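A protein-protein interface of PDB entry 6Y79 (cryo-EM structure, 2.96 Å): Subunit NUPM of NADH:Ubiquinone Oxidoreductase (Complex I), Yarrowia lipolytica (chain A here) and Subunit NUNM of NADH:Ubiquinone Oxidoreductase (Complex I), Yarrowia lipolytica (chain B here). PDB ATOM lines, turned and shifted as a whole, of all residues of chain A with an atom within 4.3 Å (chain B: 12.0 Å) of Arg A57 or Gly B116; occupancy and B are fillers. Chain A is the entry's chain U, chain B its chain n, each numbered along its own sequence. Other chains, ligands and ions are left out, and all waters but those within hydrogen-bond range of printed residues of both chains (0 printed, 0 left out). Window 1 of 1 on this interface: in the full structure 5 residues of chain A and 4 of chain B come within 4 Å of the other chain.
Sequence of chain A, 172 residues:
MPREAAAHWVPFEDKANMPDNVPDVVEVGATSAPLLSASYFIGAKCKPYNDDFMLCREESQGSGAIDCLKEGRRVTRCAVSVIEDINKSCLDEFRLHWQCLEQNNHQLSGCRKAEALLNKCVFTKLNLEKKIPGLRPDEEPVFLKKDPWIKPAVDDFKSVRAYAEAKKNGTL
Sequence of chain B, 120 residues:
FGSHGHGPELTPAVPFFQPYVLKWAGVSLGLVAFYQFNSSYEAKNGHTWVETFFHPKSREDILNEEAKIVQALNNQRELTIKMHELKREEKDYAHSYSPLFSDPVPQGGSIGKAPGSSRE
SG of Cys A68 is in hydrogen-bond range of N of Arg A57 (3.3 Å).
The side-chain sulfur (SG) of Cys A56 is disulfide-bonded to the side-chain sulfur (SG) of Cys A68 (2.0 Å).
Among the printed residues, merely in contact across the chains: Arg A57 with Gly B116, Met A54 with Pro B115, Glu A58 with Gly B116, Gly A62 with Gly B116 and Glu A58 with Ser B118.
O of Pro B115 is in hydrogen-bond range of NE of Arg A57.
No residue of chain B comes within 4 Å of Phe A53.
Of chain B, only Pro B115 (3.7 Å) comes within 4 Å of Met A54.
Leu A55 touches none of the printed residues of chain B.
No residue of chain B comes within 4 Å of Cys A56.
Of chain B, only Pro B115 (3.0 Å) and Gly B116 (3.4 Å) come within 4 Å of Arg A57.
No residue of chain B comes within 4 Å of Ser A60.
Of chain B, only Gly B116 comes within 4 Å of Gly A62.
Ala A65 touches none of the printed residues of chain B.
No residue of chain B comes within 4 Å of Cys A68.
Gln B107 touches none of the printed residues of chain A.
Of the printed residues of chain A, Pro B115 touches Met A54 and Arg A57.
Gly B116 touches just these residues of chain A: Arg A57 (3.4 Å), Glu A58 (3.8 Å) and Gly A62 (3.9 Å).
Of the printed residues of chain A, Ser B118 touches Glu A58 (3.95 Å).
The nearest printed residue of chain A that does not touch Gly B116 is Ser A60 (5.8 Å).
Of the 12 printed residues of chain A, 4 touch a printed residue of chain B.
Printed residues of chain A that touch a printed residue of chain B: Met A54, Arg A57, Glu A58 and Gly A62.
Hydrophobic or aromatic side chains of chain A within 4 Å of the printed part of chain B: Met A54.
Along chain A the printed residues that touch a printed residue of chain B span positions 54 to 62.
Printed residues of chain B that touch a printed residue of chain A: Pro B115, Gly B116 and Ser B118.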
ATOM      1  N   PHE A  53       6.378  -8.113  18.889  1.00  0.00           N
ATOM      2  CA  PHE A  53       6.941  -9.059  17.925  1.00  0.00           C
ATOM      3  C   PHE A  53       8.460  -8.942  17.847  1.00  0.00           C
ATOM      4  O   PHE A  53       9.181  -9.950  17.893  1.00  0.00           O
ATOM      5  CB  PHE A  53       6.337  -8.847  16.542  1.00  0.00           C
ATOM      6  CG  PHE A  53       6.969  -9.695  15.492  1.00  0.00           C
ATOM      7  CD1 PHE A  53       6.871 -11.070  15.556  1.00  0.00           C
ATOM      8  CD2 PHE A  53       7.679  -9.126  14.455  1.00  0.00           C
ATOM      9  CE1 PHE A  53       7.459 -11.863  14.596  1.00  0.00           C
ATOM     10  CE2 PHE A  53       8.269  -9.914  13.493  1.00  0.00           C
ATOM     11  CZ  PHE A  53       8.158 -11.284  13.564  1.00  0.00           C
ATOM     12  N   MET A  54       8.970  -7.717  17.743  1.00  0.00           N
ATOM     13  CA  MET A  54      10.421  -7.568  17.696  1.00  0.00           C
ATOM     14  C   MET A  54      11.075  -7.839  19.046  1.00  0.00           C
ATOM     15  O   MET A  54      12.223  -8.294  19.085  1.00  0.00           O
ATOM     16  CB  MET A  54      10.792  -6.182  17.169  1.00  0.00           C
ATOM     17  CG  MET A  54      10.328  -5.930  15.744  1.00  0.00           C
ATOM     18  SD  MET A  54      10.696  -7.268  14.590  1.00  0.00           S
ATOM     19  CE  MET A  54      12.361  -6.883  14.091  1.00  0.00           C
ATOM     20  N   LEU A  55      10.347  -7.648  20.146  1.00  0.00           N
ATOM     21  CA  LEU A  55      10.845  -8.020  21.461  1.00  0.00           C
ATOM     22  C   LEU A  55      10.883  -9.535  21.636  1.00  0.00           C
ATOM     23  O   LEU A  55      11.765 -10.050  22.329  1.00  0.00           O
ATOM     24  CB  LEU A  55       9.967  -7.354  22.515  1.00  0.00           C
ATOM     25  CG  LEU A  55      10.408  -7.085  23.944  1.00  0.00           C
ATOM     26  CD1 LEU A  55      11.716  -6.349  23.969  1.00  0.00           C
ATOM     27  CD2 LEU A  55       9.333  -6.253  24.609  1.00  0.00           C
ATOM     28  N   CYS A  56       9.931 -10.253  21.027  1.00  0.00           N
ATOM     29  CA  CYS A  56      10.010 -11.706  20.932  1.00  0.00           C
ATOM     30  C   CYS A  56      11.265 -12.121  20.204  1.00  0.00           C
ATOM     31  O   CYS A  56      11.976 -13.034  20.635  1.00  0.00           O
ATOM     32  CB  CYS A  56       8.783 -12.251  20.197  1.00  0.00           C
ATOM     33  SG  CYS A  56       8.819 -14.037  19.795  1.00  0.00           S
ATOM     34  N   ARG A  57      11.498 -11.508  19.043  1.00  0.00           N
ATOM     35  CA  ARG A  57      12.646 -11.855  18.220  1.00  0.00           C
ATOM     36  C   ARG A  57      13.954 -11.560  18.930  1.00  0.00           C
ATOM     37  O   ARG A  57      14.940 -12.280  18.741  1.00  0.00           O
ATOM     38  CB  ARG A  57      12.548 -11.104  16.899  1.00  0.00           C
ATOM     39  CG  ARG A  57      13.285 -11.769  15.810  1.00  0.00           C
ATOM     40  CD  ARG A  57      12.977 -11.140  14.494  1.00  0.00           C
ATOM     41  NE  ARG A  57      13.993 -11.538  13.539  1.00  0.00           N
ATOM     42  CZ  ARG A  57      13.935 -12.646  12.815  1.00  0.00           C
ATOM     43  NH1 ARG A  57      12.894 -13.456  12.923  1.00  0.00           N
ATOM     44  NH2 ARG A  57      14.917 -12.939  11.977  1.00  0.00           N
ATOM     45  N   GLU A  58      13.970 -10.534  19.772  1.00  0.00           N
ATOM     46  CA  GLU A  58      15.161 -10.292  20.562  1.00  0.00           C
ATOM     47  C   GLU A  58      15.288 -11.311  21.696  1.00  0.00           C
ATOM     48  O   GLU A  58      16.384 -11.809  21.961  1.00  0.00           O
ATOM     49  CB  GLU A  58      15.149  -8.855  21.070  1.00  0.00           C
ATOM     50  CG  GLU A  58      16.267  -8.503  22.012  1.00  0.00           C
ATOM     51  CD  GLU A  58      17.626  -8.364  21.368  1.00  0.00           C
ATOM     52  OE1 GLU A  58      18.612  -8.339  22.134  1.00  0.00           O
ATOM     53  OE2 GLU A  58      17.721  -8.240  20.129  1.00  0.00           O
ATOM     54  N   GLU A  59      14.178 -11.663  22.358  1.00  0.00           N
ATOM     55  CA  GLU A  59      14.258 -12.410  23.619  1.00  0.00           C
ATOM     56  C   GLU A  59      14.761 -13.838  23.432  1.00  0.00           C
ATOM     57  O   GLU A  59      15.668 -14.272  24.151  1.00  0.00           O
ATOM     58  CB  GLU A  59      12.905 -12.425  24.333  1.00  0.00           C
ATOM     59  CG  GLU A  59      12.973 -13.179  25.647  1.00  0.00           C
ATOM     60  CD  GLU A  59      11.731 -13.028  26.478  1.00  0.00           C
ATOM     61  OE1 GLU A  59      11.715 -13.520  27.623  1.00  0.00           O
ATOM     62  OE2 GLU A  59      10.772 -12.406  25.989  1.00  0.00           O
ATOM     63  N   SER A  60      14.195 -14.581  22.487  1.00  0.00           N
ATOM     64  CA  SER A  60      14.640 -15.943  22.204  1.00  0.00           C
ATOM     65  C   SER A  60      15.502 -15.863  20.955  1.00  0.00           C
ATOM     66  O   SER A  60      15.028 -16.027  19.833  1.00  0.00           O
ATOM     67  CB  SER A  60      13.455 -16.886  22.027  1.00  0.00           C
ATOM     68  OG  SER A  60      13.070 -17.021  20.670  1.00  0.00           O
ATOM     69  N   GLY A  62      18.105 -16.394  17.934  1.00  0.00           N
ATOM     70  CA  GLY A  62      18.481 -17.468  17.034  1.00  0.00           C
ATOM     71  C   GLY A  62      17.410 -18.470  16.645  1.00  0.00           C
ATOM     72  O   GLY A  62      17.461 -19.002  15.532  1.00  0.00           O
ATOM     73  N   GLY A  64      14.007 -17.537  16.598  1.00  0.00           N
ATOM     74  CA  GLY A  64      13.731 -16.540  15.616  1.00  0.00           C
ATOM     75  C   GLY A  64      12.386 -16.686  14.968  1.00  0.00           C
ATOM     76  O   GLY A  64      11.375 -16.132  15.405  1.00  0.00           O
ATOM     77  N   ALA A  65      12.438 -17.348  13.813  1.00  0.00           N
ATOM     78  CA  ALA A  65      11.266 -17.595  12.984  1.00  0.00           C
ATOM     79  C   ALA A  65      10.167 -18.334  13.744  1.00  0.00           C
ATOM     80  O   ALA A  65       9.085 -17.788  13.959  1.00  0.00           O
ATOM     81  CB  ALA A  65      11.693 -18.374  11.737  1.00  0.00           C
ATOM     82  N   CYS A  68       8.480 -17.023  17.153  1.00  0.00           N
ATOM     83  CA  CYS A  68       7.789 -15.735  17.119  1.00  0.00           C
ATOM     84  C   CYS A  68       6.631 -15.693  16.138  1.00  0.00           C
ATOM     85  O   CYS A  68       6.229 -14.600  15.735  1.00  0.00           O
ATOM     86  CB  CYS A  68       8.727 -14.583  16.796  1.00  0.00           C
ATOM     87  SG  CYS A  68       9.878 -14.203  18.062  1.00  0.00           S
ATOM     88  N   GLN B 107      29.675  -7.124  20.018  1.00  0.00           N
ATOM     89  CA  GLN B 107      28.466  -6.335  19.675  1.00  0.00           C
ATOM     90  C   GLN B 107      28.714  -5.293  18.578  1.00  0.00           C
ATOM     91  O   GLN B 107      28.284  -4.142  18.660  1.00  0.00           O
ATOM     92  CB  GLN B 107      27.816  -5.705  20.919  1.00  0.00           C
ATOM     93  CG  GLN B 107      28.664  -4.797  21.754  1.00  0.00           C
ATOM     94  CD  GLN B 107      27.855  -4.050  22.761  1.00  0.00           C
ATOM     95  OE1 GLN B 107      26.903  -4.589  23.336  1.00  0.00           O
ATOM     96  NE2 GLN B 107      28.174  -2.757  22.927  1.00  0.00           N
ATOM     97  N   GLY B 108      29.387  -5.719  17.513  1.00  0.00           N
ATOM     98  CA  GLY B 108      29.914  -4.804  16.518  1.00  0.00           C
ATOM     99  C   GLY B 108      29.053  -4.754  15.270  1.00  0.00           C
ATOM    100  O   GLY B 108      28.469  -5.757  14.865  1.00  0.00           O
ATOM    101  N   GLY B 109      29.016  -3.580  14.651  1.00  0.00           N
ATOM    102  CA  GLY B 109      28.252  -3.390  13.432  1.00  0.00           C
ATOM    103  C   GLY B 109      26.873  -2.801  13.657  1.00  0.00           C
ATOM    104  O   GLY B 109      25.860  -3.405  13.300  1.00  0.00           O
ATOM    105  N   GLY B 112      22.580  -1.268  10.607  1.00  0.00           N
ATOM    106  CA  GLY B 112      21.446  -1.873   9.926  1.00  0.00           C
ATOM    107  C   GLY B 112      21.052  -3.170  10.585  1.00  0.00           C
ATOM    108  O   GLY B 112      20.712  -4.151   9.917  1.00  0.00           O
ATOM    109  N   LYS B 113      21.095  -3.176  11.911  1.00  0.00           N
ATOM    110  CA  LYS B 113      21.163  -4.422  12.650  1.00  0.00           C
ATOM    111  C   LYS B 113      19.784  -5.044  12.799  1.00  0.00           C
ATOM    112  O   LYS B 113      18.766  -4.349  12.865  1.00  0.00           O
ATOM    113  CB  LYS B 113      21.839  -4.187  14.005  1.00  0.00           C
ATOM    114  CG  LYS B 113      20.948  -4.126  15.214  1.00  0.00           C
ATOM    115  CD  LYS B 113      21.751  -3.768  16.443  1.00  0.00           C
ATOM    116  CE  LYS B 113      20.887  -3.816  17.682  1.00  0.00           C
ATOM    117  NZ  LYS B 113      21.638  -3.427  18.899  1.00  0.00           N
ATOM    118  N   ALA B 114      19.763  -6.350  12.791  1.00  0.00           N
ATOM    119  CA  ALA B 114      18.595  -7.207  12.888  1.00  0.00           C
ATOM    120  C   ALA B 114      18.352  -7.566  14.342  1.00  0.00           C
ATOM    121  O   ALA B 114      19.311  -7.824  15.071  1.00  0.00           O
ATOM    122  CB  ALA B 114      18.801  -8.474  12.073  1.00  0.00           C
ATOM    123  N   PRO B 115      17.117  -7.522  14.834  1.00  0.00           N
ATOM    124  CA  PRO B 115      16.839  -8.177  16.118  1.00  0.00           C
ATOM    125  C   PRO B 115      16.813  -9.691  15.969  1.00  0.00           C
ATOM    126  O   PRO B 115      16.282 -10.230  14.997  1.00  0.00           O
ATOM    127  CB  PRO B 115      15.477  -7.604  16.518  1.00  0.00           C
ATOM    128  CG  PRO B 115      15.494  -6.247  15.891  1.00  0.00           C
ATOM    129  CD  PRO B 115      16.124  -6.474  14.549  1.00  0.00           C
ATOM    130  N   GLY B 116      17.407 -10.376  16.943  1.00  0.00           N
ATOM    131  CA  GLY B 116      17.698 -11.783  16.826  1.00  0.00           C
ATOM    132  C   GLY B 116      19.119 -12.093  16.419  1.00  0.00           C
ATOM    133  O   GLY B 116      19.423 -13.256  16.103  1.00  0.00           O
ATOM    134  N   SER B 117      19.999 -11.092  16.420  1.00  0.00           N
ATOM    135  CA  SER B 117      21.345 -11.241  15.902  1.00  0.00           C
ATOM    136  C   SER B 117      22.369 -11.483  16.998  1.00  0.00           C
ATOM    137  O   SER B 117      23.570 -11.514  16.719  1.00  0.00           O
ATOM    138  CB  SER B 117      21.723 -10.009  15.099  1.00  0.00           C
ATOM    139  OG  SER B 117      21.729  -8.882  15.965  1.00  0.00           O
ATOM    140  N   SER B 118      21.927 -11.672  18.234  1.00  0.00           N
ATOM    141  CA  SER B 118      22.841 -11.549  19.370  1.00  0.00           C
ATOM    142  C   SER B 118      23.481 -12.883  19.747  1.00  0.00           C
ATOM    143  O   SER B 118      24.688 -13.063  19.561  1.00  0.00           O
ATOM    144  CB  SER B 118      22.096 -10.920  20.547  1.00  0.00           C
ATOM    145  OG  SER B 118      21.916  -9.536  20.320  1.00  0.00           O
ATOM    146  N   ARG B 119      22.668 -13.847  20.186  1.00  0.00           N
ATOM    147  CA  ARG B 119      23.134 -15.047  20.912  1.00  0.00           C
ATOM    148  C   ARG B 119      24.109 -14.699  22.038  1.00  0.00           C
ATOM    149  O   ARG B 119      24.509 -15.560  22.816  1.00  0.00           O
ATOM    150  CB  ARG B 119      23.768 -16.065  19.964  1.00  0.00           C
ATOM    151  CG  ARG B 119      22.807 -16.789  19.052  1.00  0.00           C
ATOM    152  CD  ARG B 119      23.598 -17.617  18.067  1.00  0.00           C
ATOM    153  NE  ARG B 119      22.831 -18.694  17.492  1.00  0.00           N
ATOM    154  CZ  ARG B 119      22.309 -18.687  16.277  1.00  0.00           C
ATOM    155  NH1 ARG B 119      22.466 -17.652  15.468  1.00  0.00           N
ATOM    156  NH2 ARG B 119      21.622 -19.734  15.879  1.00  0.00           N
